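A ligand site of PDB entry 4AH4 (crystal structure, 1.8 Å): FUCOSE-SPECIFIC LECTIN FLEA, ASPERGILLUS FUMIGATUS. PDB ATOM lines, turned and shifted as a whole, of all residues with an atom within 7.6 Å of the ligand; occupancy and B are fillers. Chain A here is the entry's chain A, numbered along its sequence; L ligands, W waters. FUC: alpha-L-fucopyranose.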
ATOM      1  N   LEU A 117      -4.681  29.616  20.934  1.00  0.00           N
ATOM      2  CA  LEU A 117      -5.198  30.827  21.603  1.00  0.00           C
ATOM      3  C   LEU A 117      -5.642  31.882  20.568  1.00  0.00           C
ATOM      4  O   LEU A 117      -4.968  32.100  19.590  1.00  0.00           O
ATOM      5  CB  LEU A 117      -4.166  31.366  22.613  1.00  0.00           C
ATOM      6  CG  LEU A 117      -3.931  30.419  23.788  1.00  0.00           C
ATOM      7  CD1 LEU A 117      -2.899  30.980  24.802  1.00  0.00           C
ATOM      8  CD2 LEU A 117      -5.240  30.050  24.471  1.00  0.00           C
ATOM      9  N   GLN A 124       0.312  29.610  19.664  1.00  0.00           N
ATOM     10  CA  GLN A 124       0.245  29.237  21.055  1.00  0.00           C
ATOM     11  C   GLN A 124      -0.889  28.241  21.252  1.00  0.00           C
ATOM     12  O   GLN A 124      -2.036  28.525  20.932  1.00  0.00           O
ATOM     13  CB  GLN A 124      -0.054  30.442  21.934  1.00  0.00           C
ATOM     14  CG  GLN A 124       0.950  31.585  21.882  1.00  0.00           C
ATOM     15  CD  GLN A 124       0.559  32.731  22.816  1.00  0.00           C
ATOM     16  OE1 GLN A 124      -0.548  33.275  22.741  1.00  0.00           O
ATOM     17  NE2 GLN A 124       1.435  33.054  23.712  1.00  0.00           N
ATOM     18  N   LEU A 125      -0.562  27.104  21.807  1.00  0.00           N
ATOM     19  CA  LEU A 125      -1.456  25.977  21.941  1.00  0.00           C
ATOM     20  C   LEU A 125      -1.675  25.642  23.398  1.00  0.00           C
ATOM     21  O   LEU A 125      -0.745  25.747  24.227  1.00  0.00           O
ATOM     22  CB  LEU A 125      -0.900  24.758  21.225  1.00  0.00           C
ATOM     23  CG  LEU A 125      -0.998  24.843  19.716  1.00  0.00           C
ATOM     24  CD1 LEU A 125       0.191  24.058  19.170  1.00  0.00           C
ATOM     25  CD2 LEU A 125      -2.331  24.334  19.174  1.00  0.00           C
ATOM     26  N   ARG A 126      -2.909  25.251  23.673  1.00  0.00           N
ATOM     27  CA  ARG A 126      -3.303  24.645  24.945  1.00  0.00           C
ATOM     28  C   ARG A 126      -4.034  23.326  24.648  1.00  0.00           C
ATOM     29  O   ARG A 126      -5.095  23.313  23.958  1.00  0.00           O
ATOM     30  CB  ARG A 126      -4.165  25.579  25.793  1.00  0.00           C
ATOM     31  CG  ARG A 126      -3.531  26.938  26.151  1.00  0.00           C
ATOM     32  CD  ARG A 126      -2.293  26.765  27.032  1.00  0.00           C
ATOM     33  NE  ARG A 126      -1.709  28.051  27.434  1.00  0.00           N
ATOM     34  CZ  ARG A 126      -0.808  28.749  26.752  1.00  0.00           C
ATOM     35  NH1 ARG A 126      -0.295  28.291  25.616  1.00  0.00           N
ATOM     36  NH2 ARG A 126      -0.376  29.916  27.249  1.00  0.00           N
ATOM     37  N   TYR A 128      -5.698  19.752  26.478  1.00  0.00           N
ATOM     38  CA  TYR A 128      -6.313  19.294  27.748  1.00  0.00           C
ATOM     39  C   TYR A 128      -6.457  17.772  27.663  1.00  0.00           C
ATOM     40  O   TYR A 128      -7.021  17.260  26.685  1.00  0.00           O
ATOM     41  CB  TYR A 128      -7.655  20.009  28.082  1.00  0.00           C
ATOM     42  CG  TYR A 128      -7.461  21.510  28.123  1.00  0.00           C
ATOM     43  CD1 TYR A 128      -7.489  22.270  26.954  1.00  0.00           C
ATOM     44  CD2 TYR A 128      -7.128  22.144  29.288  1.00  0.00           C
ATOM     45  CE1 TYR A 128      -7.251  23.628  26.988  1.00  0.00           C
ATOM     46  CE2 TYR A 128      -6.828  23.492  29.333  1.00  0.00           C
ATOM     47  CZ  TYR A 128      -6.913  24.243  28.184  1.00  0.00           C
ATOM     48  OH  TYR A 128      -6.561  25.562  28.221  1.00  0.00           O
ATOM     49  N   GLU A 138      -3.658  20.763  31.835  1.00  0.00           N
ATOM     50  CA  GLU A 138      -3.340  21.558  30.685  1.00  0.00           C
ATOM     51  C   GLU A 138      -1.887  21.372  30.291  1.00  0.00           C
ATOM     52  O   GLU A 138      -0.952  21.341  31.145  1.00  0.00           O
ATOM     53  CB  GLU A 138      -3.631  23.040  30.984  1.00  0.00           C
ATOM     54  CG  GLU A 138      -3.434  24.016  29.846  1.00  0.00           C
ATOM     55  CD  GLU A 138      -3.620  25.448  30.286  1.00  0.00           C
ATOM     56  OE1 GLU A 138      -2.861  25.855  31.201  1.00  0.00           O
ATOM     57  OE2 GLU A 138      -4.514  26.171  29.732  1.00  0.00           O
ATOM     58  N   TYR A 139      -1.653  21.316  28.980  1.00  0.00           N
ATOM     59  CA  TYR A 139      -0.299  21.300  28.395  1.00  0.00           C
ATOM     60  C   TYR A 139      -0.171  22.476  27.412  1.00  0.00           C
ATOM     61  O   TYR A 139      -1.122  22.795  26.696  1.00  0.00           O
ATOM     62  CB  TYR A 139       0.005  19.936  27.708  1.00  0.00           C
ATOM     63  CG  TYR A 139      -0.228  18.729  28.590  1.00  0.00           C
ATOM     64  CD1 TYR A 139      -1.507  18.228  28.792  1.00  0.00           C
ATOM     65  CD2 TYR A 139       0.842  18.120  29.251  1.00  0.00           C
ATOM     66  CE1 TYR A 139      -1.734  17.139  29.609  1.00  0.00           C
ATOM     67  CE2 TYR A 139       0.622  17.029  30.075  1.00  0.00           C
ATOM     68  CZ  TYR A 139      -0.663  16.549  30.259  1.00  0.00           C
ATOM     69  OH  TYR A 139      -0.958  15.484  31.084  1.00  0.00           O
ATOM     70  N   MET A 140       0.997  23.157  27.423  1.00  0.00           N
ATOM     71  CA  MET A 140       1.217  24.446  26.751  1.00  0.00           C
ATOM     72  C   MET A 140       2.350  24.426  25.784  1.00  0.00           C
ATOM     73  O   MET A 140       3.421  23.857  26.082  1.00  0.00           O
ATOM     74  CB  MET A 140       1.617  25.515  27.745  1.00  0.00           C
ATOM     75  CG  MET A 140       0.632  25.799  28.854  1.00  0.00           C
ATOM     76  SD  MET A 140       1.186  27.254  29.782  1.00  0.00           S
ATOM     77  CE  MET A 140       2.704  26.697  30.549  1.00  0.00           C
ATOM     78  N   ASN A 142       4.217  27.552  23.973  1.00  0.00           N
ATOM     79  CA  ASN A 142       4.393  28.978  23.702  1.00  0.00           C
ATOM     80  C   ASN A 142       5.682  29.333  22.927  1.00  0.00           C
ATOM     81  O   ASN A 142       6.304  30.356  23.202  1.00  0.00           O
ATOM     82  CB  ASN A 142       4.346  29.724  25.005  1.00  0.00           C
ATOM     83  CG  ASN A 142       3.004  29.624  25.708  1.00  0.00           C
ATOM     84  OD1 ASN A 142       1.930  30.005  25.171  1.00  0.00           O
ATOM     85  ND2 ASN A 142       3.059  29.168  26.929  1.00  0.00           N
ATOM     86  N   GLU A 148       4.004  21.560  30.943  1.00  0.00           N
ATOM     87  CA  GLU A 148       2.740  21.536  31.709  1.00  0.00           C
ATOM     88  C   GLU A 148       2.273  22.923  32.128  1.00  0.00           C
ATOM     89  O   GLU A 148       3.085  23.758  32.516  1.00  0.00           O
ATOM     90  CB  GLU A 148       2.823  20.594  32.934  1.00  0.00           C
ATOM     91  CG  GLU A 148       3.108  19.154  32.529  1.00  0.00           C
ATOM     92  CD  GLU A 148       2.827  18.099  33.566  1.00  0.00           C
ATOM     93  OE1 GLU A 148       1.895  18.235  34.384  1.00  0.00           O
ATOM     94  OE2 GLU A 148       3.547  17.067  33.533  1.00  0.00           O
ATOM     95  N   GLY A 149       0.986  23.189  31.976  1.00  0.00           N
ATOM     96  CA  GLY A 149       0.331  24.397  32.417  1.00  0.00           C
ATOM     97  C   GLY A 149      -0.444  24.130  33.682  1.00  0.00           C
ATOM     98  O   GLY A 149       0.008  23.390  34.525  1.00  0.00           O
ATOM     99  N   THR A 150      -1.624  24.710  33.792  1.00  0.00           N
ATOM    100  CA  THR A 150      -2.444  24.632  34.994  1.00  0.00           C
ATOM    101  C   THR A 150      -3.132  23.265  35.127  1.00  0.00           C
ATOM    102  O   THR A 150      -3.686  22.760  34.141  1.00  0.00           O
ATOM    103  CB  THR A 150      -3.488  25.739  35.010  1.00  0.00           C
ATOM    104  OG1 THR A 150      -2.856  27.015  34.844  1.00  0.00           O
ATOM    105  CG2 THR A 150      -4.253  25.773  36.327  1.00  0.00           C
ATOM    106  N   ASN A 151      -3.097  22.676  36.330  1.00  0.00           N
ATOM    107  CA  ASN A 151      -3.958  21.517  36.641  1.00  0.00           C
ATOM    108  C   ASN A 151      -5.373  21.975  37.021  1.00  0.00           C
ATOM    109  O   ASN A 151      -5.542  22.875  37.848  1.00  0.00           O
ATOM    110  CB  ASN A 151      -3.363  20.620  37.733  1.00  0.00           C
ATOM    111  CG  ASN A 151      -4.091  19.305  37.828  1.00  0.00           C
ATOM    112  OD1 ASN A 151      -5.200  19.233  38.366  1.00  0.00           O
ATOM    113  ND2 ASN A 151      -3.543  18.291  37.205  1.00  0.00           N
ATOM    114  N   LEU A 152      -6.387  21.410  36.372  1.00  0.00           N
ATOM    115  CA  LEU A 152      -7.767  21.896  36.557  1.00  0.00           C
ATOM    116  C   LEU A 152      -8.666  20.993  37.389  1.00  0.00           C
ATOM    117  O   LEU A 152      -9.874  21.210  37.490  1.00  0.00           O
ATOM    118  CB  LEU A 152      -8.375  22.246  35.203  1.00  0.00           C
ATOM    119  CG  LEU A 152      -7.552  23.299  34.433  1.00  0.00           C
ATOM    120  CD1 LEU A 152      -7.998  23.456  32.992  1.00  0.00           C
ATOM    121  CD2 LEU A 152      -7.556  24.648  35.129  1.00  0.00           C
ATOM    122  N   PRO A 174      -6.239  36.500  25.327  1.00  0.00           N
ATOM    123  CA  PRO A 174      -7.250  35.485  25.012  1.00  0.00           C
ATOM    124  C   PRO A 174      -7.967  34.929  26.233  1.00  0.00           C
ATOM    125  O   PRO A 174      -7.404  34.927  27.352  1.00  0.00           O
ATOM    126  CB  PRO A 174      -6.445  34.380  24.342  1.00  0.00           C
ATOM    127  CG  PRO A 174      -5.113  34.495  24.966  1.00  0.00           C
ATOM    128  CD  PRO A 174      -4.864  35.989  25.196  1.00  0.00           C
ATOM    129  N   SER A 175      -9.185  34.433  26.030  1.00  0.00           N
ATOM    130  CA  SER A 175      -9.915  33.664  27.044  1.00  0.00           C
ATOM    131  C   SER A 175     -10.004  32.200  26.632  1.00  0.00           C
ATOM    132  O   SER A 175      -9.826  31.873  25.470  1.00  0.00           O
ATOM    133  CB  SER A 175     -11.297  34.195  27.237  1.00  0.00           C
ATOM    134  OG  SER A 175     -11.276  35.502  27.746  1.00  0.00           O
ATOM    135  N   ILE A 176     -10.216  31.337  27.604  1.00  0.00           N
ATOM    136  CA  ILE A 176     -10.359  29.890  27.358  1.00  0.00           C
ATOM    137  C   ILE A 176     -11.572  29.443  28.106  1.00  0.00           C
ATOM    138  O   ILE A 176     -11.812  29.860  29.217  1.00  0.00           O
ATOM    139  CB  ILE A 176      -9.135  29.040  27.773  1.00  0.00           C
ATOM    140  CG1 ILE A 176      -7.815  29.626  27.247  1.00  0.00           C
ATOM    141  CG2 ILE A 176      -9.306  27.608  27.224  1.00  0.00           C
ATOM    142  CD1 ILE A 176      -6.584  29.006  27.916  1.00  0.00           C
ATOM    143  N   TYR A 192     -11.127  30.522  31.959  1.00  0.00           N
ATOM    144  CA  TYR A 192      -9.919  31.308  32.072  1.00  0.00           C
ATOM    145  C   TYR A 192     -10.103  32.675  31.356  1.00  0.00           C
ATOM    146  O   TYR A 192     -10.379  32.705  30.132  1.00  0.00           O
ATOM    147  CB  TYR A 192      -8.723  30.584  31.425  1.00  0.00           C
ATOM    148  CG  TYR A 192      -7.467  31.432  31.482  1.00  0.00           C
ATOM    149  CD1 TYR A 192      -7.193  32.367  30.496  1.00  0.00           C
ATOM    150  CD2 TYR A 192      -6.569  31.322  32.552  1.00  0.00           C
ATOM    151  CE1 TYR A 192      -6.095  33.199  30.590  1.00  0.00           C
ATOM    152  CE2 TYR A 192      -5.464  32.150  32.640  1.00  0.00           C
ATOM    153  CZ  TYR A 192      -5.239  33.071  31.654  1.00  0.00           C
ATOM    154  OH  TYR A 192      -4.136  33.886  31.715  1.00  0.00           O
ATOM    155  N   ASP A 193      -9.893  33.757  32.105  1.00  0.00           N
ATOM    156  CA  ASP A 193      -9.805  35.117  31.567  1.00  0.00           C
ATOM    157  C   ASP A 193      -8.470  35.722  32.031  1.00  0.00           C
ATOM    158  O   ASP A 193      -7.922  35.314  33.083  1.00  0.00           O
ATOM    159  CB  ASP A 193     -10.960  36.008  32.035  1.00  0.00           C
ATOM    160  CG  ASP A 193     -12.265  35.746  31.325  1.00  0.00           C
ATOM    161  OD1 ASP A 193     -12.257  35.241  30.158  1.00  0.00           O
ATOM    162  OD2 ASP A 193     -13.347  36.096  31.921  1.00  0.00           O
ATOM    163  N   PRO A 194      -7.915  36.683  31.248  1.00  0.00           N
ATOM    164  CA  PRO A 194      -6.611  37.210  31.593  1.00  0.00           C
ATOM    165  C   PRO A 194      -6.566  37.953  32.951  1.00  0.00           C
ATOM    166  O   PRO A 194      -5.511  38.008  33.535  1.00  0.00           O
ATOM    167  CB  PRO A 194      -6.245  38.146  30.425  1.00  0.00           C
ATOM    168  CG  PRO A 194      -7.421  38.234  29.545  1.00  0.00           C
ATOM    169  CD  PRO A 194      -8.372  37.111  29.911  1.00  0.00           C
ATOM    170  N   GLY A 197      -7.523  34.799  35.743  1.00  0.00           N
ATOM    171  CA  GLY A 197      -6.890  33.518  35.518  1.00  0.00           C
ATOM    172  C   GLY A 197      -7.993  32.467  35.432  1.00  0.00           C
ATOM    173  O   GLY A 197      -9.093  32.735  34.938  1.00  0.00           O
ATOM    174  N   TRP A 198      -7.727  31.270  35.935  1.00  0.00           N
ATOM    175  CA  TRP A 198      -8.795  30.259  36.023  1.00  0.00           C
ATOM    176  C   TRP A 198      -9.732  30.563  37.161  1.00  0.00           C
ATOM    177  O   TRP A 198      -9.295  30.597  38.312  1.00  0.00           O
ATOM    178  CB  TRP A 198      -8.187  28.838  36.152  1.00  0.00           C
ATOM    179  CG  TRP A 198      -7.545  28.375  34.894  1.00  0.00           C
ATOM    180  CD1 TRP A 198      -6.190  28.389  34.561  1.00  0.00           C
ATOM    181  CD2 TRP A 198      -8.214  27.832  33.723  1.00  0.00           C
ATOM    182  NE1 TRP A 198      -6.024  27.904  33.292  1.00  0.00           N
ATOM    183  CE2 TRP A 198      -7.185  27.560  32.750  1.00  0.00           C
ATOM    184  CE3 TRP A 198      -9.538  27.548  33.393  1.00  0.00           C
ATOM    185  CZ2 TRP A 198      -7.486  27.024  31.509  1.00  0.00           C
ATOM    186  CZ3 TRP A 198      -9.819  27.024  32.137  1.00  0.00           C
ATOM    187  CH2 TRP A 198      -8.809  26.774  31.210  1.00  0.00           C
HETATM  188  C1  FUC L   1      -0.708  30.357  30.952  1.00  0.00           C
HETATM  189  C2  FUC L   1      -1.301  29.106  31.602  1.00  0.00           C
HETATM  190  C3  FUC L   1      -2.797  29.218  31.876  1.00  0.00           C
HETATM  191  C4  FUC L   1      -3.466  29.668  30.576  1.00  0.00           C
HETATM  192  C5  FUC L   1      -2.789  30.900  29.997  1.00  0.00           C
HETATM  193  C6  FUC L   1      -3.425  31.304  28.663  1.00  0.00           C
HETATM  194  O1  FUC L   1      -0.721  31.476  31.828  1.00  0.00           O
HETATM  195  O2  FUC L   1      -0.578  28.816  32.804  1.00  0.00           O
HETATM  196  O3  FUC L   1      -3.362  27.976  32.333  1.00  0.00           O
HETATM  197  O4  FUC L   1      -3.377  28.659  29.589  1.00  0.00           O
HETATM  198  O5  FUC L   1      -1.408  30.651  29.759  1.00  0.00           O
HETATM  199  O   HOH W   1      -1.287  30.554  35.021  1.00  0.00           O
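The side-chain carboxylate (OE1) of Glu 138 lies within hydrogen-bond range of an oxygen (O3) of the ligand (2.5 Å).
NE of Arg 126 lies within hydrogen-bond range of O4 of the ligand (2.8 Å).
O3 of the ligand sits at hydrogen-bond distance from OG1 of Thr 150, 2.7 Å away.
The indole nitrogen (NE1) of Trp 198 sits at hydrogen-bond distance from an oxygen (O3) of the ligand, 2.8 Å away.
The guanidinium group (NH1) of Arg 126 is in hydrogen-bond range of the side-chain amide oxygen (OD1) of Asn 142, at 2.8 Å.
The backbone NH (N) of Glu 138 is in hydrogen-bond range of the backbone carbonyl oxygen (O) of Thr 150 (3.1 Å).
OH of Tyr 128 is in hydrogen-bond range of OE2 of Glu 138 (2.6 Å).
The backbone NH of Gly 149 sits at hydrogen-bond distance from the backbone carbonyl oxygen of Glu 138.
O of Tyr 192 is in hydrogen-bond range of N of Ile 176 (2.9 Å).
N of Leu 117 sits at hydrogen-bond distance from O of Gln 124, at 2.9 Å.
Merely in contact with the ligand: Leu 117, Met 140, Ile 176 and Tyr 192.
Hydrophobic or aromatic side chains within 4 Å of the ligand: Leu 117, Met 140, Ile 176, Tyr 192 and Trp 198.
Within 4 Å of the ligand: Leu 117, Arg 126, Glu 138, Met 140, Thr 150, Ile 176, Tyr 192 and Trp 198.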
